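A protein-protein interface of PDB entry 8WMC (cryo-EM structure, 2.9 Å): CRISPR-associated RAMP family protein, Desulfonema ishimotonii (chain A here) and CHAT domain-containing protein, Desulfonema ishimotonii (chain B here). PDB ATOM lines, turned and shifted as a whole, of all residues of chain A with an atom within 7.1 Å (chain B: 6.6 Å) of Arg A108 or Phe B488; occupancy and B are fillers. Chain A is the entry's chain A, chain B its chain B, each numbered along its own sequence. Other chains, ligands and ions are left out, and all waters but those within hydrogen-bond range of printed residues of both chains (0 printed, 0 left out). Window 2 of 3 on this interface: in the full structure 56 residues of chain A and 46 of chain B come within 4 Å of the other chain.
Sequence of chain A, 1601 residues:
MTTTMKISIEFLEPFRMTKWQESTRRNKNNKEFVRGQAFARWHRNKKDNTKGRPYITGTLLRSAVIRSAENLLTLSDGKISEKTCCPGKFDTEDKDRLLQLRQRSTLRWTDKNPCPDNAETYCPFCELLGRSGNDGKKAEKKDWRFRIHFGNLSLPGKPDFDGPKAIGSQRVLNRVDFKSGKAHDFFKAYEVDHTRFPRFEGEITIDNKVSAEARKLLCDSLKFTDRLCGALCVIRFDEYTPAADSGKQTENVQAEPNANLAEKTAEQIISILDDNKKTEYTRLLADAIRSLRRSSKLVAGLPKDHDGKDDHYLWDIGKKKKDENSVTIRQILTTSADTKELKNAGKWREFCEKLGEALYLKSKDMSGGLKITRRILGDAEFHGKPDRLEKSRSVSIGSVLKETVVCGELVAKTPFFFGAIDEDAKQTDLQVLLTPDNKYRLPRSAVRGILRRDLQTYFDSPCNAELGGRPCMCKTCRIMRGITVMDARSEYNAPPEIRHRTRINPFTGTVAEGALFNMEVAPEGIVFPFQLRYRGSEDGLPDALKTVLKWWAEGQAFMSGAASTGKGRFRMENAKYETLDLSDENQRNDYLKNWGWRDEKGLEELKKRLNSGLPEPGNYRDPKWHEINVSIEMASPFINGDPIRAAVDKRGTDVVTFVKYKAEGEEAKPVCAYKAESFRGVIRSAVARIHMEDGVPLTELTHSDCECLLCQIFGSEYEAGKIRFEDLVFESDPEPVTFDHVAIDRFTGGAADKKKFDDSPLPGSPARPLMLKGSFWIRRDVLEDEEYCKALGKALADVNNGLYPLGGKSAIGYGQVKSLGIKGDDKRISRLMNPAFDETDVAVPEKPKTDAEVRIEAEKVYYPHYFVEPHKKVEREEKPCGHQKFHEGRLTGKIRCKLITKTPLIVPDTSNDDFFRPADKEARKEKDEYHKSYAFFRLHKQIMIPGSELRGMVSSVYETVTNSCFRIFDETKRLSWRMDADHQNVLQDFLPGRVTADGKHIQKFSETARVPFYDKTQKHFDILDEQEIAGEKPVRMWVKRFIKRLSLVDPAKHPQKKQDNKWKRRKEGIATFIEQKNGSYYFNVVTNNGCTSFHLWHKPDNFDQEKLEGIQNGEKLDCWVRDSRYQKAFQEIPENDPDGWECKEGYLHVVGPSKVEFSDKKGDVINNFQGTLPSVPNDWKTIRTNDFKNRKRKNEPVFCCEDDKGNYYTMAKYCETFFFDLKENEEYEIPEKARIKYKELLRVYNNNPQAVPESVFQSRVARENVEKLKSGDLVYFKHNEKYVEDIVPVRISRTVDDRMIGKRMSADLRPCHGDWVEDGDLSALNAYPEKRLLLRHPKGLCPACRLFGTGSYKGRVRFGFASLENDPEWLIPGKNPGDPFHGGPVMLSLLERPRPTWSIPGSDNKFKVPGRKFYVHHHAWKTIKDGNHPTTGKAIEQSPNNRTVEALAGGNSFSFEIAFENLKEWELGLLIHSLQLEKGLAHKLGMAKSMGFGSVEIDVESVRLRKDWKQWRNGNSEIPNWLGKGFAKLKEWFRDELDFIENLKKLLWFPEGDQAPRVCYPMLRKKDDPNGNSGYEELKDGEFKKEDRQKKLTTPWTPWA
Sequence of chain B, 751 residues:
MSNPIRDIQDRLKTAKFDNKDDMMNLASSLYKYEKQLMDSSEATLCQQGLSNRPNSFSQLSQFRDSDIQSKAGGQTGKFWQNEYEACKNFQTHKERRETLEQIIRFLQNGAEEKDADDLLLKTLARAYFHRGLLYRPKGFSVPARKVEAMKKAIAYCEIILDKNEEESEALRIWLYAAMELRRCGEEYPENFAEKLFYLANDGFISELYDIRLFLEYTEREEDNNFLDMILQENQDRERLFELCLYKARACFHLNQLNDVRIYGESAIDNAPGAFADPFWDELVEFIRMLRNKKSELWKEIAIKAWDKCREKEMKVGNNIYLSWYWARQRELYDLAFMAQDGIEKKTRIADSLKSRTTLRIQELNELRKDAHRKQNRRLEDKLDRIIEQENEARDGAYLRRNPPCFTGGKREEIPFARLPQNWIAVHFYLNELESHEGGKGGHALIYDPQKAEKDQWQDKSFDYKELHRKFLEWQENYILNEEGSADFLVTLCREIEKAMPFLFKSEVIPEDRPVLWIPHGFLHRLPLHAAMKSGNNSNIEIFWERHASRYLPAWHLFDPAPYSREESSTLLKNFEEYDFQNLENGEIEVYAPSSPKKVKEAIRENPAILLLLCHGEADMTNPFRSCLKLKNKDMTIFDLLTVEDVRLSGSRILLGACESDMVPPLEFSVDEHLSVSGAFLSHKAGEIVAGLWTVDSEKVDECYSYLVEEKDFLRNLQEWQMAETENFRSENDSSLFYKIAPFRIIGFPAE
The backbone NH of Ser A396 is in hydrogen-bond range of the side-chain amide oxygen of Asn B477 (3.4 Å).
Of chain B, only Phe B488 (3.9 Å) comes within 4 Å of Arg A108. Of the printed residues of chain B, Ser A394 touches Glu B473 (3.8 Å) and Asn B477 (3.8 Å). Of the printed residues of chain B, Ser A396 touches Asn B477 and Asn B481. Of the printed residues of chain A, Glu B473 touches Ser A394. Of the printed residues of chain A, Asn B477 touches Ser A394, Val A395 and Ser A396. Ala B486 touches none of the printed residues of chain A. Of chain A, only Arg A108 (3.9 Å) comes within 4 Å of Phe B488. The nearest residue of chain A that does not touch Phe B488 is Ser A394 (4.4 Å).
Among the printed residues, merely in contact across the chains: Val A395 with Asn B477, Ser A396 with Asn B481, Ser A394 with Glu B473, Ser A394 with Asn B477 and Arg A108 with Phe B488.
Hydrophobic or aromatic side chains of chain B that line the printed part of chain A: Phe B488. Printed residues of chain A that touch a printed residue of chain B: Arg A108, Ser A394, Val A395 and Ser A396. Hydrophobic or aromatic side chains of chain A that line the printed part of chain B: Val A395. Among the printed residues, no Asp or Glu carboxylate lies within 4 Å of a Lys or Arg side-chain nitrogen of the other chain.
The backbone carbonyl oxygen of Glu B473 sits at hydrogen-bond distance from the side-chain amide nitrogen of Asn B477, at 3.1 Å. The side-chain amide oxygen (OD1) of Asn B481 sits close to the backbone carbonyl oxygen (O) of Asn B477. O of Gly B484 lies within hydrogen-bond range of ND2 of Asn B481 (3.2 Å). The backbone carbonyl oxygen (O) of Thr A106 sits at hydrogen-bond distance from the backbone NH (N) of Val A395, at 3.0 Å. The guanidinium group (NH2) of Arg A108 lies within salt-bridge range of the side-chain carboxylate (OD1) of Asp A111 (2.9 Å). The backbone carbonyl oxygen (O) of Val A395 lies within hydrogen-bond range of the backbone NH (N) of Arg A108.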
ATOM      1  N   GLU A  70      18.337  -7.774  19.204  1.00  0.00           N
ATOM      2  CA  GLU A  70      17.679  -8.297  18.009  1.00  0.00           C
ATOM      3  C   GLU A  70      16.545  -7.383  17.562  1.00  0.00           C
ATOM      4  O   GLU A  70      16.390  -7.111  16.363  1.00  0.00           O
ATOM      5  CB  GLU A  70      17.155  -9.707  18.275  1.00  0.00           C
ATOM      6  CG  GLU A  70      18.109 -10.806  17.847  1.00  0.00           C
ATOM      7  CD  GLU A  70      17.474 -12.177  17.883  1.00  0.00           C
ATOM      8  OE1 GLU A  70      16.670 -12.440  18.801  1.00  0.00           O
ATOM      9  OE2 GLU A  70      17.783 -12.993  16.992  1.00  0.00           O
ATOM     10  N   THR A  74      16.481  -5.432  13.901  1.00  0.00           N
ATOM     11  CA  THR A  74      15.428  -5.535  12.892  1.00  0.00           C
ATOM     12  C   THR A  74      14.757  -4.189  12.652  1.00  0.00           C
ATOM     13  O   THR A  74      14.306  -3.918  11.534  1.00  0.00           O
ATOM     14  CB  THR A  74      14.387  -6.599  13.267  1.00  0.00           C
ATOM     15  OG1 THR A  74      13.412  -6.699  12.222  1.00  0.00           O
ATOM     16  CG2 THR A  74      13.680  -6.285  14.573  1.00  0.00           C
ATOM     17  N   PRO A  87      22.981 -12.632  10.695  1.00  0.00           N
ATOM     18  CA  PRO A  87      21.872 -13.031  11.577  1.00  0.00           C
ATOM     19  C   PRO A  87      22.291 -13.847  12.792  1.00  0.00           C
ATOM     20  O   PRO A  87      21.417 -14.254  13.566  1.00  0.00           O
ATOM     21  CB  PRO A  87      20.965 -13.850  10.647  1.00  0.00           C
ATOM     22  CG  PRO A  87      21.866 -14.381   9.617  1.00  0.00           C
ATOM     23  CD  PRO A  87      22.930 -13.350   9.407  1.00  0.00           C
ATOM     24  N   SER A 105      10.324 -17.832  17.808  1.00  0.00           N
ATOM     25  CA  SER A 105      10.804 -17.678  16.441  1.00  0.00           C
ATOM     26  C   SER A 105      11.789 -16.518  16.382  1.00  0.00           C
ATOM     27  O   SER A 105      11.453 -15.391  16.761  1.00  0.00           O
ATOM     28  CB  SER A 105       9.636 -17.440  15.488  1.00  0.00           C
ATOM     29  OG  SER A 105      10.097 -17.216  14.169  1.00  0.00           O
ATOM     30  N   THR A 106      13.000 -16.793  15.905  1.00  0.00           N
ATOM     31  CA  THR A 106      14.032 -15.770  15.832  1.00  0.00           C
ATOM     32  C   THR A 106      13.679 -14.728  14.776  1.00  0.00           C
ATOM     33  O   THR A 106      13.094 -15.037  13.735  1.00  0.00           O
ATOM     34  CB  THR A 106      15.387 -16.405  15.513  1.00  0.00           C
ATOM     35  OG1 THR A 106      15.604 -17.530  16.374  1.00  0.00           O
ATOM     36  CG2 THR A 106      16.513 -15.410  15.720  1.00  0.00           C
ATOM     37  N   LEU A 107      14.038 -13.478  15.055  1.00  0.00           N
ATOM     38  CA  LEU A 107      13.775 -12.391  14.125  1.00  0.00           C
ATOM     39  C   LEU A 107      14.760 -12.430  12.963  1.00  0.00           C
ATOM     40  O   LEU A 107      15.916 -12.834  13.114  1.00  0.00           O
ATOM     41  CB  LEU A 107      13.858 -11.043  14.841  1.00  0.00           C
ATOM     42  CG  LEU A 107      12.923 -10.856  16.041  1.00  0.00           C
ATOM     43  CD1 LEU A 107      13.132  -9.495  16.676  1.00  0.00           C
ATOM     44  CD2 LEU A 107      11.468 -11.027  15.639  1.00  0.00           C
ATOM     45  N   ARG A 108      14.285 -11.996  11.795  1.00  0.00           N
ATOM     46  CA  ARG A 108      15.035 -12.060  10.548  1.00  0.00           C
ATOM     47  C   ARG A 108      15.107 -10.671   9.932  1.00  0.00           C
ATOM     48  O   ARG A 108      14.087  -9.985   9.825  1.00  0.00           O
ATOM     49  CB  ARG A 108      14.376 -13.037   9.568  1.00  0.00           C
ATOM     50  CG  ARG A 108      15.299 -13.584   8.492  1.00  0.00           C
ATOM     51  CD  ARG A 108      14.817 -14.939   8.002  1.00  0.00           C
ATOM     52  NE  ARG A 108      15.539 -15.389   6.818  1.00  0.00           N
ATOM     53  CZ  ARG A 108      15.291 -14.990   5.577  1.00  0.00           C
ATOM     54  NH1 ARG A 108      14.346 -14.103   5.303  1.00  0.00           N
ATOM     55  NH2 ARG A 108      16.015 -15.491   4.579  1.00  0.00           N
ATOM     56  N   TRP A 109      16.317 -10.264   9.534  1.00  0.00           N
ATOM     57  CA  TRP A 109      16.523  -8.981   8.875  1.00  0.00           C
ATOM     58  C   TRP A 109      17.479  -9.043   7.690  1.00  0.00           C
ATOM     59  O   TRP A 109      17.718  -8.005   7.067  1.00  0.00           O
ATOM     60  CB  TRP A 109      17.036  -7.938   9.886  1.00  0.00           C
ATOM     61  CG  TRP A 109      18.356  -8.278  10.526  1.00  0.00           C
ATOM     62  CD1 TRP A 109      19.599  -8.082   9.998  1.00  0.00           C
ATOM     63  CD2 TRP A 109      18.558  -8.862  11.819  1.00  0.00           C
ATOM     64  NE1 TRP A 109      20.561  -8.514  10.878  1.00  0.00           N
ATOM     65  CE2 TRP A 109      19.948  -8.996  12.003  1.00  0.00           C
ATOM     66  CE3 TRP A 109      17.699  -9.287  12.836  1.00  0.00           C
ATOM     67  CZ2 TRP A 109      20.498  -9.537  13.162  1.00  0.00           C
ATOM     68  CZ3 TRP A 109      18.248  -9.823  13.986  1.00  0.00           C
ATOM     69  CH2 TRP A 109      19.634  -9.943  14.139  1.00  0.00           C
ATOM     70  N   THR A 110      18.030 -10.209   7.358  1.00  0.00           N
ATOM     71  CA  THR A 110      18.982 -10.317   6.260  1.00  0.00           C
ATOM     72  C   THR A 110      18.990 -11.751   5.751  1.00  0.00           C
ATOM     73  O   THR A 110      18.530 -12.671   6.431  1.00  0.00           O
ATOM     74  CB  THR A 110      20.391  -9.882   6.689  1.00  0.00           C
ATOM     75  OG1 THR A 110      21.303 -10.070   5.600  1.00  0.00           O
ATOM     76  CG2 THR A 110      20.878 -10.675   7.902  1.00  0.00           C
ATOM     77  N   ASP A 111      19.532 -11.924   4.543  1.00  0.00           N
ATOM     78  CA  ASP A 111      19.584 -13.214   3.866  1.00  0.00           C
ATOM     79  C   ASP A 111      20.988 -13.806   3.810  1.00  0.00           C
ATOM     80  O   ASP A 111      21.185 -14.836   3.156  1.00  0.00           O
ATOM     81  CB  ASP A 111      19.028 -13.078   2.447  1.00  0.00           C
ATOM     82  CG  ASP A 111      17.579 -12.634   2.428  1.00  0.00           C
ATOM     83  OD1 ASP A 111      16.829 -13.001   3.355  1.00  0.00           O
ATOM     84  OD2 ASP A 111      17.190 -11.915   1.484  1.00  0.00           O
ATOM     85  N   LYS A 112      21.967 -13.193   4.474  1.00  0.00           N
ATOM     86  CA  LYS A 112      23.337 -13.687   4.462  1.00  0.00           C
ATOM     87  C   LYS A 112      23.533 -14.729   5.554  1.00  0.00           C
ATOM     88  O   LYS A 112      22.947 -14.633   6.636  1.00  0.00           O
ATOM     89  CB  LYS A 112      24.327 -12.537   4.653  1.00  0.00           C
ATOM     90  CG  LYS A 112      24.007 -11.303   3.827  1.00  0.00           C
ATOM     91  CD  LYS A 112      25.187 -10.348   3.765  1.00  0.00           C
ATOM     92  CE  LYS A 112      24.903  -9.174   2.843  1.00  0.00           C
ATOM     93  NZ  LYS A 112      26.124  -8.367   2.571  1.00  0.00           N
ATOM     94  N   SER A 394      12.477 -19.009  11.788  1.00  0.00           N
ATOM     95  CA  SER A 394      12.892 -17.619  11.653  1.00  0.00           C
ATOM     96  C   SER A 394      11.863 -16.886  10.807  1.00  0.00           C
ATOM     97  O   SER A 394      11.486 -17.370   9.736  1.00  0.00           O
ATOM     98  CB  SER A 394      14.282 -17.512  11.017  1.00  0.00           C
ATOM     99  OG  SER A 394      14.239 -17.850   9.643  1.00  0.00           O
ATOM    100  N   VAL A 395      11.417 -15.726  11.289  1.00  0.00           N
ATOM    101  CA  VAL A 395      10.386 -14.934  10.629  1.00  0.00           C
ATOM    102  C   VAL A 395      10.837 -13.483  10.568  1.00  0.00           C
ATOM    103  O   VAL A 395      11.647 -13.027  11.381  1.00  0.00           O
ATOM    104  CB  VAL A 395       9.019 -15.045  11.347  1.00  0.00           C
ATOM    105  CG1 VAL A 395       8.533 -16.486  11.346  1.00  0.00           C
ATOM    106  CG2 VAL A 395       9.095 -14.495  12.774  1.00  0.00           C
ATOM    107  N   SER A 396      10.294 -12.755   9.591  1.00  0.00           N
ATOM    108  CA  SER A 396      10.570 -11.336   9.388  1.00  0.00           C
ATOM    109  C   SER A 396       9.276 -10.567   9.629  1.00  0.00           C
ATOM    110  O   SER A 396       8.324 -10.686   8.850  1.00  0.00           O
ATOM    111  CB  SER A 396      11.106 -11.083   7.982  1.00  0.00           C
ATOM    112  OG  SER A 396      10.047 -10.941   7.051  1.00  0.00           O
ATOM    113  N   ILE A 397       9.247  -9.775  10.701  1.00  0.00           N
ATOM    114  CA  ILE A 397       8.034  -9.049  11.068  1.00  0.00           C
ATOM    115  C   ILE A 397       7.885  -7.723  10.328  1.00  0.00           C
ATOM    116  O   ILE A 397       6.757  -7.226  10.197  1.00  0.00           O
ATOM    117  CB  ILE A 397       7.980  -8.814  12.591  1.00  0.00           C
ATOM    118  CG1 ILE A 397       9.091  -7.863  13.064  1.00  0.00           C
ATOM    119  CG2 ILE A 397       8.076 -10.143  13.327  1.00  0.00           C
ATOM    120  CD1 ILE A 397       9.186  -7.745  14.572  1.00  0.00           C
ATOM    121  N   GLY A 398       8.979  -7.141   9.845  1.00  0.00           N
ATOM    122  CA  GLY A 398       8.962  -5.880   9.129  1.00  0.00           C
ATOM    123  C   GLY A 398       9.619  -4.771   9.935  1.00  0.00           C
ATOM    124  O   GLY A 398       9.970  -4.928  11.106  1.00  0.00           O
ATOM    125  N   LYS B 470      10.160 -26.449   7.143  1.00  0.00           N
ATOM    126  CA  LYS B 470       9.921 -25.400   6.156  1.00  0.00           C
ATOM    127  C   LYS B 470       8.446 -25.028   6.099  1.00  0.00           C
ATOM    128  O   LYS B 470       8.103 -23.849   5.943  1.00  0.00           O
ATOM    129  CB  LYS B 470      10.418 -25.847   4.779  1.00  0.00           C
ATOM    130  CG  LYS B 470      11.932 -26.066   4.666  1.00  0.00           C
ATOM    131  CD  LYS B 470      12.746 -24.802   4.949  1.00  0.00           C
ATOM    132  CE  LYS B 470      14.242 -25.024   4.757  1.00  0.00           C
ATOM    133  NZ  LYS B 470      14.598 -25.549   3.408  1.00  0.00           N
ATOM    134  N   GLU B 473       7.729 -22.772   9.056  1.00  0.00           N
ATOM    135  CA  GLU B 473       8.265 -21.431   8.833  1.00  0.00           C
ATOM    136  C   GLU B 473       7.386 -20.644   7.867  1.00  0.00           C
ATOM    137  O   GLU B 473       7.066 -19.470   8.110  1.00  0.00           O
ATOM    138  CB  GLU B 473       9.696 -21.519   8.307  1.00  0.00           C
ATOM    139  CG  GLU B 473      10.749 -21.632   9.400  1.00  0.00           C
ATOM    140  CD  GLU B 473      12.165 -21.500   8.875  1.00  0.00           C
ATOM    141  OE1 GLU B 473      12.352 -20.922   7.784  1.00  0.00           O
ATOM    142  OE2 GLU B 473      13.097 -21.977   9.556  1.00  0.00           O
ATOM    143  N   TRP B 474       6.978 -21.279   6.763  1.00  0.00           N
ATOM    144  CA  TRP B 474       6.126 -20.593   5.798  1.00  0.00           C
ATOM    145  C   TRP B 474       4.783 -20.231   6.411  1.00  0.00           C
ATOM    146  O   TRP B 474       4.245 -19.154   6.142  1.00  0.00           O
ATOM    147  CB  TRP B 474       5.913 -21.455   4.556  1.00  0.00           C
ATOM    148  CG  TRP B 474       4.881 -20.875   3.630  1.00  0.00           C
ATOM    149  CD1 TRP B 474       5.068 -19.875   2.723  1.00  0.00           C
ATOM    150  CD2 TRP B 474       3.502 -21.253   3.530  1.00  0.00           C
ATOM    151  NE1 TRP B 474       3.895 -19.608   2.062  1.00  0.00           N
ATOM    152  CE2 TRP B 474       2.917 -20.440   2.540  1.00  0.00           C
ATOM    153  CE3 TRP B 474       2.707 -22.198   4.183  1.00  0.00           C
ATOM    154  CZ2 TRP B 474       1.576 -20.546   2.184  1.00  0.00           C
ATOM    155  CZ3 TRP B 474       1.373 -22.302   3.828  1.00  0.00           C
ATOM    156  CH2 TRP B 474       0.822 -21.481   2.838  1.00  0.00           C
ATOM    157  N   ASN B 477       5.245 -17.174   8.692  1.00  0.00           N
ATOM    158  CA  ASN B 477       5.415 -15.958   7.899  1.00  0.00           C
ATOM    159  C   ASN B 477       4.105 -15.534   7.245  1.00  0.00           C
ATOM    160  O   ASN B 477       3.765 -14.346   7.233  1.00  0.00           O
ATOM    161  CB  ASN B 477       6.494 -16.170   6.839  1.00  0.00           C
ATOM    162  CG  ASN B 477       7.892 -16.005   7.394  1.00  0.00           C
ATOM    163  OD1 ASN B 477       8.204 -14.999   8.030  1.00  0.00           O
ATOM    164  ND2 ASN B 477       8.740 -16.999   7.166  1.00  0.00           N
ATOM    165  N   ASN B 481       2.778 -11.691   7.982  1.00  0.00           N
ATOM    166  CA  ASN B 481       2.795 -10.612   6.995  1.00  0.00           C
ATOM    167  C   ASN B 481       2.050 -10.957   5.706  1.00  0.00           C
ATOM    168  O   ASN B 481       2.185 -10.237   4.713  1.00  0.00           O
ATOM    169  CB  ASN B 481       4.239 -10.192   6.688  1.00  0.00           C
ATOM    170  CG  ASN B 481       5.067 -11.296   6.044  1.00  0.00           C
ATOM    171  OD1 ASN B 481       4.566 -12.361   5.697  1.00  0.00           O
ATOM    172  ND2 ASN B 481       6.359 -11.032   5.885  1.00  0.00           N
ATOM    173  N   GLY B 484       3.983 -11.401   2.143  1.00  0.00           N
ATOM    174  CA  GLY B 484       5.432 -11.347   2.158  1.00  0.00           C
ATOM    175  C   GLY B 484       6.090 -12.682   2.449  1.00  0.00           C
ATOM    176  O   GLY B 484       7.047 -12.745   3.226  1.00  0.00           O
ATOM    177  N   SER B 485       5.582 -13.758   1.830  1.00  0.00           N
ATOM    178  CA  SER B 485       6.133 -15.094   2.025  1.00  0.00           C
ATOM    179  C   SER B 485       6.176 -15.894   0.724  1.00  0.00           C
ATOM    180  O   SER B 485       6.219 -17.131   0.770  1.00  0.00           O
ATOM    181  CB  SER B 485       5.321 -15.855   3.076  1.00  0.00           C
ATOM    182  OG  SER B 485       3.965 -15.971   2.683  1.00  0.00           O
ATOM    183  N   ALA B 486       6.169 -15.225  -0.432  1.00  0.00           N
ATOM    184  CA  ALA B 486       6.224 -15.943  -1.702  1.00  0.00           C
ATOM    185  C   ALA B 486       7.544 -16.687  -1.857  1.00  0.00           C
ATOM    186  O   ALA B 486       7.576 -17.817  -2.359  1.00  0.00           O
ATOM    187  CB  ALA B 486       6.015 -14.970  -2.860  1.00  0.00           C
ATOM    188  N   ASP B 487       8.649 -16.066  -1.438  1.00  0.00           N
ATOM    189  CA  ASP B 487       9.935 -16.754  -1.471  1.00  0.00           C
ATOM    190  C   ASP B 487       9.929 -17.969  -0.551  1.00  0.00           C
ATOM    191  O   ASP B 487      10.522 -19.006  -0.871  1.00  0.00           O
ATOM    192  CB  ASP B 487      11.064 -15.794  -1.091  1.00  0.00           C
ATOM    193  CG  ASP B 487      10.849 -15.140   0.260  1.00  0.00           C
ATOM    194  OD1 ASP B 487       9.770 -15.337   0.855  1.00  0.00           O
ATOM    195  OD2 ASP B 487      11.762 -14.425   0.727  1.00  0.00           O
ATOM    196  N   PHE B 488       9.263 -17.861   0.600  1.00  0.00           N
ATOM    197  CA  PHE B 488       9.152 -19.008   1.494  1.00  0.00           C
ATOM    198  C   PHE B 488       8.335 -20.126   0.856  1.00  0.00           C
ATOM    199  O   PHE B 488       8.654 -21.309   1.021  1.00  0.00           O
ATOM    200  CB  PHE B 488       8.540 -18.575   2.825  1.00  0.00           C
ATOM    201  CG  PHE B 488       9.497 -17.834   3.712  1.00  0.00           C
ATOM    202  CD1 PHE B 488      10.375 -18.521   4.531  1.00  0.00           C
ATOM    203  CD2 PHE B 488       9.527 -16.451   3.719  1.00  0.00           C
ATOM    204  CE1 PHE B 488      11.260 -17.842   5.345  1.00  0.00           C
ATOM    205  CE2 PHE B 488      10.408 -15.767   4.531  1.00  0.00           C
ATOM    206  CZ  PHE B 488      11.277 -16.463   5.343  1.00  0.00           C
ATOM    207  N   LEU B 489       7.275 -19.773   0.124  1.00  0.00           N
ATOM    208  CA  LEU B 489       6.510 -20.786  -0.599  1.00  0.00           C
ATOM    209  C   LEU B 489       7.365 -21.459  -1.669  1.00  0.00           C
ATOM    210  O   LEU B 489       7.276 -22.677  -1.878  1.00  0.00           O
ATOM    211  CB  LEU B 489       5.266 -20.151  -1.222  1.00  0.00           C
ATOM    212  CG  LEU B 489       4.305 -21.072  -1.979  1.00  0.00           C
ATOM    213  CD1 LEU B 489       3.713 -22.122  -1.055  1.00  0.00           C
ATOM    214  CD2 LEU B 489       3.202 -20.258  -2.634  1.00  0.00           C
ATOM    215  N   VAL B 490       8.189 -20.675  -2.367  1.00  0.00           N
ATOM    216  CA  VAL B 490       9.100 -21.240  -3.361  1.00  0.00           C
ATOM    217  C   VAL B 490      10.073 -22.209  -2.700  1.00  0.00           C
ATOM    218  O   VAL B 490      10.346 -23.298  -3.225  1.00  0.00           O
ATOM    219  CB  VAL B 490       9.837 -20.108  -4.105  1.00  0.00           C
ATOM    220  CG1 VAL B 490      11.029 -20.644  -4.899  1.00  0.00           C
ATOM    221  CG2 VAL B 490       8.875 -19.363  -5.023  1.00  0.00           C
ATOM    222  N   THR B 491      10.611 -21.827  -1.542  1.00  0.00           N
ATOM    223  CA  THR B 491      11.509 -22.714  -0.812  1.00  0.00           C
ATOM    224  C   THR B 491      10.792 -23.990  -0.388  1.00  0.00           C
ATOM    225  O   THR B 491      11.374 -25.079  -0.424  1.00  0.00           O
ATOM    226  CB  THR B 491      12.081 -21.993   0.409  1.00  0.00           C
ATOM    227  OG1 THR B 491      12.859 -20.868  -0.018  1.00  0.00           O
ATOM    228  CG2 THR B 491      12.959 -22.929   1.226  1.00  0.00           C
ATOM    229  N   LEU B 492       9.527 -23.872   0.021  1.00  0.00           N
ATOM    230  CA  LEU B 492       8.756 -25.051   0.405  1.00  0.00           C
ATOM    231  C   LEU B 492       8.571 -25.999  -0.772  1.00  0.00           C
ATOM    232  O   LEU B 492       8.704 -27.220  -0.624  1.00  0.00           O
ATOM    233  CB  LEU B 492       7.398 -24.624   0.960  1.00  0.00           C
ATOM    234  CG  LEU B 492       6.599 -25.705   1.692  1.00  0.00           C
ATOM    235  CD1 LEU B 492       7.208 -25.995   3.051  1.00  0.00           C
ATOM    236  CD2 LEU B 492       5.145 -25.283   1.831  1.00  0.00           C
ATOM    237  N   CYS B 493       8.253 -25.458  -1.947  1.00  0.00           N
ATOM    238  CA  CYS B 493       8.088 -26.306  -3.125  1.00  0.00           C
ATOM    239  C   CYS B 493       9.402 -26.979  -3.512  1.00  0.00           C
ATOM    240  O   CYS B 493       9.424 -28.163  -3.883  1.00  0.00           O
ATOM    241  CB  CYS B 493       7.542 -25.479  -4.285  1.00  0.00           C
ATOM    242  SG  CYS B 493       5.791 -25.060  -4.132  1.00  0.00           S
ATOM    243  N   SER B 734       8.037 -14.650  -8.186  1.00  0.00           N
ATOM    244  CA  SER B 734       7.548 -15.426  -7.052  1.00  0.00           C
ATOM    245  C   SER B 734       6.211 -14.892  -6.555  1.00  0.00           C
ATOM    246  O   SER B 734       5.338 -15.664  -6.141  1.00  0.00           O
ATOM    247  CB  SER B 734       8.583 -15.411  -5.928  1.00  0.00           C
ATOM    248  OG  SER B 734       8.127 -16.139  -4.802  1.00  0.00           O
